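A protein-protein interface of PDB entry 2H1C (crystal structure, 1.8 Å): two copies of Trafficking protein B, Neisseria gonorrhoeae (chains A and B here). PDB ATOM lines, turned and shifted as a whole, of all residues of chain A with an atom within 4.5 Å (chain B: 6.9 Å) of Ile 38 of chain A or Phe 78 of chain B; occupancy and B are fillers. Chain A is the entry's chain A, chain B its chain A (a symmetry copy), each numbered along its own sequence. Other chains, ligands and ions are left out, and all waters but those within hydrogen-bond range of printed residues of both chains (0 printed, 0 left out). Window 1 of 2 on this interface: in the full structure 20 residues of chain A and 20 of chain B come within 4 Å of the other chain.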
ATOM      1  N   SER A  36      21.049  -2.454  31.065  1.00  0.00           N
ATOM      2  CA  SER A  36      20.225  -1.802  30.051  1.00  0.00           C
ATOM      3  C   SER A  36      20.921  -2.063  28.729  1.00  0.00           C
ATOM      4  O   SER A  36      22.154  -2.134  28.679  1.00  0.00           O
ATOM      5  CB  SER A  36      20.176  -0.289  30.268  1.00  0.00           C
ATOM      6  OG  SER A  36      19.829   0.371  29.050  1.00  0.00           O
ATOM      7  N   ALA A  37      20.147  -2.197  27.658  1.00  0.00           N
ATOM      8  CA  ALA A  37      20.735  -2.394  26.349  1.00  0.00           C
ATOM      9  C   ALA A  37      21.649  -1.190  26.024  1.00  0.00           C
ATOM     10  O   ALA A  37      22.595  -1.308  25.254  1.00  0.00           O
ATOM     11  CB  ALA A  37      19.621  -2.530  25.298  1.00  0.00           C
ATOM     12  N   ILE A  38      21.359  -0.035  26.620  1.00  0.00           N
ATOM     13  CA  ILE A  38      22.171   1.179  26.418  1.00  0.00           C
ATOM     14  C   ILE A  38      23.596   0.971  26.971  1.00  0.00           C
ATOM     15  O   ILE A  38      24.583   1.362  26.347  1.00  0.00           O
ATOM     16  CB  ILE A  38      21.531   2.416  27.138  1.00  0.00           C
ATOM     17  CG1 ILE A  38      20.197   2.785  26.462  1.00  0.00           C
ATOM     18  CG2 ILE A  38      22.498   3.602  27.119  1.00  0.00           C
ATOM     19  CD1 ILE A  38      20.328   3.291  25.029  1.00  0.00           C
ATOM     20  N   THR A  39      23.688   0.367  28.157  1.00  0.00           N
ATOM     21  CA  THR A  39      24.972   0.079  28.797  1.00  0.00           C
ATOM     22  C   THR A  39      25.738  -0.966  27.981  1.00  0.00           C
ATOM     23  O   THR A  39      26.951  -0.862  27.809  1.00  0.00           O
ATOM     24  CB  THR A  39      24.742  -0.418  30.245  1.00  0.00           C
ATOM     25  OG1 THR A  39      24.045   0.603  30.963  1.00  0.00           O
ATOM     26  CG2 THR A  39      26.053  -0.719  30.942  1.00  0.00           C
ATOM     27  N   VAL A  40      25.030  -1.965  27.459  1.00  0.00           N
ATOM     28  CA  VAL A  40      25.681  -2.992  26.656  1.00  0.00           C
ATOM     29  C   VAL A  40      26.256  -2.319  25.407  1.00  0.00           C
ATOM     30  O   VAL A  40      27.365  -2.643  24.974  1.00  0.00           O
ATOM     31  CB  VAL A  40      24.690  -4.116  26.245  1.00  0.00           C
ATOM     32  CG1 VAL A  40      25.370  -5.097  25.305  1.00  0.00           C
ATOM     33  CG2 VAL A  40      24.199  -4.870  27.504  1.00  0.00           C
ATOM     34  N   ALA A  41      25.519  -1.367  24.837  1.00  0.00           N
ATOM     35  CA  ALA A  41      26.015  -0.668  23.645  1.00  0.00           C
ATOM     36  C   ALA A  41      27.284   0.124  23.976  1.00  0.00           C
ATOM     37  O   ALA A  41      28.239   0.157  23.182  1.00  0.00           O
ATOM     38  CB  ALA A  41      24.959   0.277  23.116  1.00  0.00           C
ATOM     39  N   GLU A  42      27.284   0.792  25.127  1.00  0.00           N
ATOM     40  CA  GLU A  42      28.445   1.586  25.524  1.00  0.00           C
ATOM     41  C   GLU A  42      29.643   0.698  25.836  1.00  0.00           C
ATOM     42  O   GLU A  42      30.778   1.061  25.518  1.00  0.00           O
ATOM     43  CB  GLU A  42      28.122   2.470  26.734  1.00  0.00           C
ATOM     44  CG  GLU A  42      26.886   3.345  26.540  1.00  0.00           C
ATOM     45  CD  GLU A  42      26.593   4.231  27.738  1.00  0.00           C
ATOM     46  OE1 GLU A  42      26.930   3.816  28.877  1.00  0.00           O
ATOM     47  OE2 GLU A  42      26.011   5.330  27.545  1.00  0.00           O
ATOM     48  N   PRO A  77      15.557  -3.700  27.197  1.00  0.00           N
ATOM     49  CA  PRO A  77      15.519  -2.728  26.094  1.00  0.00           C
ATOM     50  C   PRO A  77      14.944  -1.358  26.437  1.00  0.00           C
ATOM     51  O   PRO A  77      14.263  -1.190  27.449  1.00  0.00           O
ATOM     52  CB  PRO A  77      14.673  -3.449  25.033  1.00  0.00           C
ATOM     53  CG  PRO A  77      13.665  -4.189  25.875  1.00  0.00           C
ATOM     54  CD  PRO A  77      14.543  -4.756  27.015  1.00  0.00           C
ATOM     55  N   PHE A  78      15.267  -0.362  25.609  1.00  0.00           N
ATOM     56  CA  PHE A  78      14.692   0.965  25.785  1.00  0.00           C
ATOM     57  C   PHE A  78      13.522   0.882  24.783  1.00  0.00           C
ATOM     58  O   PHE A  78      13.724   1.007  23.574  1.00  0.00           O
ATOM     59  CB  PHE A  78      15.658   2.082  25.353  1.00  0.00           C
ATOM     60  CG  PHE A  78      15.122   3.467  25.612  1.00  0.00           C
ATOM     61  CD1 PHE A  78      15.296   4.079  26.857  1.00  0.00           C
ATOM     62  CD2 PHE A  78      14.369   4.129  24.643  1.00  0.00           C
ATOM     63  CE1 PHE A  78      14.723   5.337  27.132  1.00  0.00           C
ATOM     64  CE2 PHE A  78      13.791   5.383  24.903  1.00  0.00           C
ATOM     65  CZ  PHE A  78      13.966   5.990  26.145  1.00  0.00           C
ATOM     66  N   TYR A 106      18.212   7.670  29.967  1.00  0.00           N
ATOM     67  CA  TYR A 106      17.784   6.366  29.432  1.00  0.00           C
ATOM     68  C   TYR A 106      17.880   5.275  30.491  1.00  0.00           C
ATOM     69  O   TYR A 106      16.980   4.439  30.637  1.00  0.00           O
ATOM     70  CB  TYR A 106      18.650   5.950  28.247  1.00  0.00           C
ATOM     71  CG  TYR A 106      18.502   6.843  27.048  1.00  0.00           C
ATOM     72  CD1 TYR A 106      19.580   7.084  26.205  1.00  0.00           C
ATOM     73  CD2 TYR A 106      17.283   7.459  26.762  1.00  0.00           C
ATOM     74  CE1 TYR A 106      19.452   7.925  25.098  1.00  0.00           C
ATOM     75  CE2 TYR A 106      17.142   8.303  25.657  1.00  0.00           C
ATOM     76  CZ  TYR A 106      18.233   8.531  24.833  1.00  0.00           C
ATOM     77  OH  TYR A 106      18.105   9.382  23.755  1.00  0.00           O
ATOM     78  N   SER B  36      11.546   4.895  16.032  1.00  0.00           N
ATOM     79  CA  SER B  36      12.398   4.283  17.048  1.00  0.00           C
ATOM     80  C   SER B  36      11.844   4.749  18.381  1.00  0.00           C
ATOM     81  O   SER B  36      11.339   5.873  18.486  1.00  0.00           O
ATOM     82  CB  SER B  36      13.839   4.782  16.936  1.00  0.00           C
ATOM     83  OG  SER B  36      14.519   4.604  18.179  1.00  0.00           O
ATOM     84  N   ALA B  37      11.942   3.904  19.402  1.00  0.00           N
ATOM     85  CA  ALA B  37      11.486   4.294  20.721  1.00  0.00           C
ATOM     86  C   ALA B  37      12.271   5.547  21.172  1.00  0.00           C
ATOM     87  O   ALA B  37      11.789   6.334  21.978  1.00  0.00           O
ATOM     88  CB  ALA B  37      11.702   3.132  21.705  1.00  0.00           C
ATOM     89  N   ILE B  38      13.481   5.722  20.646  1.00  0.00           N
ATOM     90  CA  ILE B  38      14.318   6.892  20.971  1.00  0.00           C
ATOM     91  C   ILE B  38      13.645   8.188  20.475  1.00  0.00           C
ATOM     92  O   ILE B  38      13.631   9.204  21.171  1.00  0.00           O
ATOM     93  CB  ILE B  38      15.735   6.778  20.308  1.00  0.00           C
ATOM     94  CG1 ILE B  38      16.519   5.615  20.944  1.00  0.00           C
ATOM     95  CG2 ILE B  38      16.498   8.095  20.457  1.00  0.00           C
ATOM     96  CD1 ILE B  38      16.876   5.814  22.413  1.00  0.00           C
ATOM     97  N   LEU B  76       9.919   0.786  17.331  1.00  0.00           N
ATOM     98  CA  LEU B  76      11.039  -0.142  17.503  1.00  0.00           C
ATOM     99  C   LEU B  76      11.940   0.089  18.700  1.00  0.00           C
ATOM    100  O   LEU B  76      12.496   1.166  18.860  1.00  0.00           O
ATOM    101  CB  LEU B  76      11.886  -0.124  16.237  1.00  0.00           C
ATOM    102  CG  LEU B  76      11.103  -0.385  14.935  1.00  0.00           C
ATOM    103  CD1 LEU B  76      11.996  -0.100  13.733  1.00  0.00           C
ATOM    104  CD2 LEU B  76      10.615  -1.824  14.934  1.00  0.00           C
ATOM    105  N   PRO B  77      12.141  -0.941  19.535  1.00  0.00           N
ATOM    106  CA  PRO B  77      13.008  -0.713  20.700  1.00  0.00           C
ATOM    107  C   PRO B  77      14.508  -0.745  20.426  1.00  0.00           C
ATOM    108  O   PRO B  77      14.955  -1.252  19.396  1.00  0.00           O
ATOM    109  CB  PRO B  77      12.583  -1.830  21.666  1.00  0.00           C
ATOM    110  CG  PRO B  77      12.290  -2.972  20.726  1.00  0.00           C
ATOM    111  CD  PRO B  77      11.505  -2.271  19.594  1.00  0.00           C
ATOM    112  N   PHE B  78      15.284  -0.153  21.336  1.00  0.00           N
ATOM    113  CA  PHE B  78      16.736  -0.212  21.226  1.00  0.00           C
ATOM    114  C   PHE B  78      17.024  -1.404  22.162  1.00  0.00           C
ATOM    115  O   PHE B  78      17.010  -1.256  23.385  1.00  0.00           O
ATOM    116  CB  PHE B  78      17.416   1.051  21.781  1.00  0.00           C
ATOM    117  CG  PHE B  78      18.911   1.053  21.593  1.00  0.00           C
ATOM    118  CD1 PHE B  78      19.482   1.517  20.404  1.00  0.00           C
ATOM    119  CD2 PHE B  78      19.750   0.514  22.569  1.00  0.00           C
ATOM    120  CE1 PHE B  78      20.872   1.443  20.190  1.00  0.00           C
ATOM    121  CE2 PHE B  78      21.138   0.432  22.369  1.00  0.00           C
ATOM    122  CZ  PHE B  78      21.703   0.895  21.183  1.00  0.00           C
ATOM    123  N   ASP B  79      17.244  -2.580  21.583  1.00  0.00           N
ATOM    124  CA  ASP B  79      17.494  -3.792  22.359  1.00  0.00           C
ATOM    125  C   ASP B  79      18.909  -4.349  22.168  1.00  0.00           C
ATOM    126  O   ASP B  79      19.752  -3.709  21.551  1.00  0.00           O
ATOM    127  CB  ASP B  79      16.461  -4.858  21.987  1.00  0.00           C
ATOM    128  CG  ASP B  79      16.414  -5.125  20.494  1.00  0.00           C
ATOM    129  OD1 ASP B  79      17.359  -4.710  19.786  1.00  0.00           O
ATOM    130  OD2 ASP B  79      15.432  -5.752  20.028  1.00  0.00           O
ATOM    131  N   GLU B  80      19.174  -5.541  22.691  1.00  0.00           N
ATOM    132  CA  GLU B  80      20.516  -6.115  22.574  1.00  0.00           C
ATOM    133  C   GLU B  80      21.096  -6.219  21.159  1.00  0.00           C
ATOM    134  O   GLU B  80      22.256  -5.873  20.934  1.00  0.00           O
ATOM    135  CB  GLU B  80      20.573  -7.476  23.285  1.00  0.00           C
ATOM    136  CG  GLU B  80      21.952  -8.129  23.273  1.00  0.00           C
ATOM    137  CD  GLU B  80      22.253  -8.830  21.969  1.00  0.00           C
ATOM    138  OE1 GLU B  80      21.352  -9.524  21.457  1.00  0.00           O
ATOM    139  OE2 GLU B  80      23.389  -8.699  21.459  1.00  0.00           O
ATOM    140  N   PRO B  81      20.312  -6.707  20.185  1.00  0.00           N
ATOM    141  CA  PRO B  81      20.817  -6.822  18.809  1.00  0.00           C
ATOM    142  C   PRO B  81      21.180  -5.448  18.225  1.00  0.00           C
ATOM    143  O   PRO B  81      22.178  -5.298  17.513  1.00  0.00           O
ATOM    144  CB  PRO B  81      19.642  -7.464  18.064  1.00  0.00           C
ATOM    145  CG  PRO B  81      18.979  -8.277  19.127  1.00  0.00           C
ATOM    146  CD  PRO B  81      18.999  -7.361  20.320  1.00  0.00           C
ATOM    147  N   VAL B  82      20.353  -4.454  18.517  1.00  0.00           N
ATOM    148  CA  VAL B  82      20.595  -3.095  18.027  1.00  0.00           C
ATOM    149  C   VAL B  82      21.855  -2.526  18.691  1.00  0.00           C
ATOM    150  O   VAL B  82      22.617  -1.775  18.071  1.00  0.00           O
ATOM    151  CB  VAL B  82      19.418  -2.166  18.330  1.00  0.00           C
ATOM    152  CG1 VAL B  82      19.680  -0.786  17.730  1.00  0.00           C
ATOM    153  CG2 VAL B  82      18.140  -2.753  17.757  1.00  0.00           C
ATOM    154  N   ALA B  83      22.065  -2.877  19.957  1.00  0.00           N
ATOM    155  CA  ALA B  83      23.249  -2.412  20.665  1.00  0.00           C
ATOM    156  C   ALA B  83      24.522  -2.892  19.964  1.00  0.00           C
ATOM    157  O   ALA B  83      25.507  -2.163  19.892  1.00  0.00           O
ATOM    158  CB  ALA B  83      23.225  -2.897  22.120  1.00  0.00           C
ATOM    159  N   ALA B  84      24.511  -4.120  19.453  1.00  0.00           N
ATOM    160  CA  ALA B  84      25.677  -4.658  18.748  1.00  0.00           C
ATOM    161  C   ALA B  84      25.972  -3.846  17.495  1.00  0.00           C
ATOM    162  O   ALA B  84      27.124  -3.516  17.206  1.00  0.00           O
ATOM    163  CB  ALA B  84      25.445  -6.126  18.365  1.00  0.00           C
ATOM    164  N   TYR B  86      25.034  -0.803  16.932  1.00  0.00           N
ATOM    165  CA  TYR B  86      25.425   0.530  17.370  1.00  0.00           C
ATOM    166  C   TYR B  86      26.940   0.629  17.566  1.00  0.00           C
ATOM    167  O   TYR B  86      27.579   1.535  17.039  1.00  0.00           O
ATOM    168  CB  TYR B  86      24.728   0.864  18.687  1.00  0.00           C
ATOM    169  CG  TYR B  86      25.244   2.110  19.373  1.00  0.00           C
ATOM    170  CD1 TYR B  86      24.770   3.376  19.021  1.00  0.00           C
ATOM    171  CD2 TYR B  86      26.201   2.017  20.385  1.00  0.00           C
ATOM    172  CE1 TYR B  86      25.238   4.524  19.666  1.00  0.00           C
ATOM    173  CE2 TYR B  86      26.668   3.142  21.027  1.00  0.00           C
ATOM    174  CZ  TYR B  86      26.186   4.391  20.668  1.00  0.00           C
ATOM    175  OH  TYR B  86      26.637   5.516  21.315  1.00  0.00           O
ATOM    176  N   ALA B  87      27.509  -0.295  18.340  1.00  0.00           N
ATOM    177  CA  ALA B  87      28.938  -0.276  18.610  1.00  0.00           C
ATOM    178  C   ALA B  87      29.731  -0.426  17.322  1.00  0.00           C
ATOM    179  O   ALA B  87      30.737   0.257  17.127  1.00  0.00           O
ATOM    180  CB  ALA B  87      29.301  -1.382  19.591  1.00  0.00           C
ATOM    181  N   ALA B 102      25.915   9.967  19.637  1.00  0.00           N
ATOM    182  CA  ALA B 102      25.181   8.843  20.229  1.00  0.00           C
ATOM    183  C   ALA B 102      23.724   8.759  19.755  1.00  0.00           C
ATOM    184  O   ALA B 102      23.274   7.704  19.300  1.00  0.00           O
ATOM    185  CB  ALA B 102      25.227   8.936  21.763  1.00  0.00           C
ATOM    186  N   GLY B 105      23.422   7.722  16.360  1.00  0.00           N
ATOM    187  CA  GLY B 105      23.867   6.347  16.313  1.00  0.00           C
ATOM    188  C   GLY B 105      22.758   5.377  16.691  1.00  0.00           C
ATOM    189  O   GLY B 105      22.644   4.316  16.088  1.00  0.00           O
ATOM    190  N   TYR B 106      21.953   5.717  17.697  1.00  0.00           N
ATOM    191  CA  TYR B 106      20.861   4.823  18.118  1.00  0.00           C
ATOM    192  C   TYR B 106      19.859   4.604  16.991  1.00  0.00           C
ATOM    193  O   TYR B 106      19.405   3.481  16.744  1.00  0.00           O
ATOM    194  CB  TYR B 106      20.109   5.403  19.312  1.00  0.00           C
ATOM    195  CG  TYR B 106      20.937   5.493  20.561  1.00  0.00           C
ATOM    196  CD1 TYR B 106      20.740   6.526  21.470  1.00  0.00           C
ATOM    197  CD2 TYR B 106      21.931   4.551  20.831  1.00  0.00           C
ATOM    198  CE1 TYR B 106      21.518   6.625  22.626  1.00  0.00           C
ATOM    199  CE2 TYR B 106      22.715   4.638  21.984  1.00  0.00           C
ATOM    200  CZ  TYR B 106      22.502   5.680  22.873  1.00  0.00           C
ATOM    201  OH  TYR B 106      23.291   5.784  24.001  1.00  0.00           O
ATOM    202  N   ILE B 107      19.508   5.699  16.326  1.00  0.00           N
ATOM    203  CA  ILE B 107      18.557   5.656  15.228  1.00  0.00           C
ATOM    204  C   ILE B 107      19.140   4.898  14.058  1.00  0.00           C
ATOM    205  O   ILE B 107      18.474   4.039  13.491  1.00  0.00           O
ATOM    206  CB  ILE B 107      18.160   7.075  14.805  1.00  0.00           C
ATOM    207  CG1 ILE B 107      17.481   7.777  15.986  1.00  0.00           C
ATOM    208  CG2 ILE B 107      17.196   7.020  13.633  1.00  0.00           C
ATOM    209  CD1 ILE B 107      17.090   9.199  15.718  1.00  0.00           C
ATOM    210  N   ALA B 109      21.444   2.574  14.037  1.00  0.00           N
ATOM    211  CA  ALA B 109      21.550   1.143  14.344  1.00  0.00           C
ATOM    212  C   ALA B 109      20.179   0.454  14.275  1.00  0.00           C
ATOM    213  O   ALA B 109      20.073  -0.695  13.840  1.00  0.00           O
ATOM    214  CB  ALA B 109      22.174   0.939  15.744  1.00  0.00           C
ATOM    215  N   THR B 110      19.132   1.155  14.700  1.00  0.00           N
ATOM    216  CA  THR B 110      17.780   0.600  14.651  1.00  0.00           C
ATOM    217  C   THR B 110      17.392   0.368  13.192  1.00  0.00           C
ATOM    218  O   THR B 110      16.891  -0.694  12.833  1.00  0.00           O
ATOM    219  CB  THR B 110      16.753   1.555  15.322  1.00  0.00           C
ATOM    220  OG1 THR B 110      17.093   1.722  16.710  1.00  0.00           O
ATOM    221  CG2 THR B 110      15.327   0.988  15.203  1.00  0.00           C
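Hydrophobic or aromatic side chains of chain B that line the printed part of chain A: Ala 37, Ile 38, Pro 77, Phe 78, Ala 83, Tyr 86 and Tyr 106.
Along chain B the printed residues that touch a printed residue of chain A span positions 37 to 106.
Hydrophobic or aromatic side chains of chain A that line the printed part of chain B: Ala 37, Ile 38, Ala 41, Pro 77, Phe 78 and Tyr 106.
Among the printed residues, 16 pairs touch across the chains.
Among the printed residues, no Asp or Glu carboxylate lies within 4 Å of a Lys or Arg side-chain nitrogen of the other chain.
Of chain B, only Phe 78 (3.8 Å) and Tyr 106 (3.9 Å) come within 4 Å of Ile 38 of chain A.
Of the printed residues of chain A, Phe 78 of chain B touches Ala 37 (3.5 Å), Ile 38 (3.8 Å), Ala 41 (3.8 Å), Pro 77 (3.4 Å) and Phe 78 (3.0 Å).
Of the printed residues of chain A, Tyr 106 of chain B touches Ile 38 (3.9 Å) and Tyr 106 (3.5 Å).
Of the printed residues of chain B, Tyr 106 of chain A touches Ile 38 and Tyr 106.
Of the printed residues of chain A, Ala 83 of chain B touches Ala 37 (3.6 Å) and Ala 41 (3.8 Å).
Printed residues of chain B within 4 Å of Ala 41 of chain A: Phe 78 (3.8 Å), Ala 83 (3.8 Å) and Tyr 86 (3.5 Å).
Of the printed residues of chain B, Ala 37 of chain A touches Phe 78 (3.5 Å), Asp 79 (3.7 Å) and Ala 83 (3.6 Å).
The nearest residue of chain B that does not touch Ile 38 of chain A is Ile 38 of chain B (5.0 Å).
Among the printed residues, merely in contact across the chains: Ala 37 of chain A with Phe 78 of chain B (3.5 Å), Ala 37 of chain A with Asp 79 of chain B (3.7 Å), Ala 37 of chain A with Ala 83 of chain B (3.6 Å), Ile 38 of chain A with Phe 78 of chain B (3.8 Å), Ile 38 of chain A with Tyr 106 of chain B (3.9 Å), Ala 41 of chain A with Phe 78 of chain B (3.8 Å), Ala 41 of chain A with Ala 83 of chain B (3.8 Å), Ala 41 of chain A with Tyr 86 of chain B (3.5 Å), Pro 77 of chain A with Phe 78 of chain B (3.4 Å), Pro 77 of chain A with Asp 79 of chain B (3.8 Å), Phe 78 of chain A with Ala 37 of chain B (3.5 Å), Phe 78 of chain A with Ile 38 of chain B (3.8 Å), Phe 78 of chain A with Pro 77 of chain B (3.4 Å), Tyr 106 of chain A with Ile 38 of chain B (3.9 Å) and Tyr 106 of chain A with Tyr 106 of chain B (3.5 Å).
The side-chain hydroxyl (OG) of Ser 36 of chain A lies close to the backbone NH (N) of Ile 38 of chain A.
The backbone NH (N) of Ile 38 of chain B sits close to the side-chain hydroxyl (OG) of Ser 36 of chain B (2.9 Å).
The backbone carbonyl oxygen (O) of Leu 76 of chain B lies within hydrogen-bond range of the backbone NH (N) of Ala 37 of chain B (2.8 Å).
The side-chain carboxylate of Asp 79 of chain B sits close to the backbone NH of Val 82 of chain B.
O of Tyr 106 of chain B is in hydrogen-bond range of OG1 of Thr 110 of chain B.
O of Phe 78 of chain B lies within hydrogen-bond range of N of Phe 78 of chain A.
Ile 38 of chain A touches Phe 78 of chain B, and with the chains exchanged Phe 78 of chain A touches Ile 38 of chain B.
Pro 77 of chain A touches Phe 78 of chain B, and with the chains exchanged Phe 78 of chain A touches Pro 77 of chain B.
Phe 78 of chain A touches its own counterpart, Phe 78 of chain B.
Tyr 106 of chain B touches its own counterpart, Tyr 106 of chain A.
6 positions are printed for both chains.
Of the 16 pairs that touch across the chains among the printed residues, 10 have their exchanged pair printed and touching as well.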
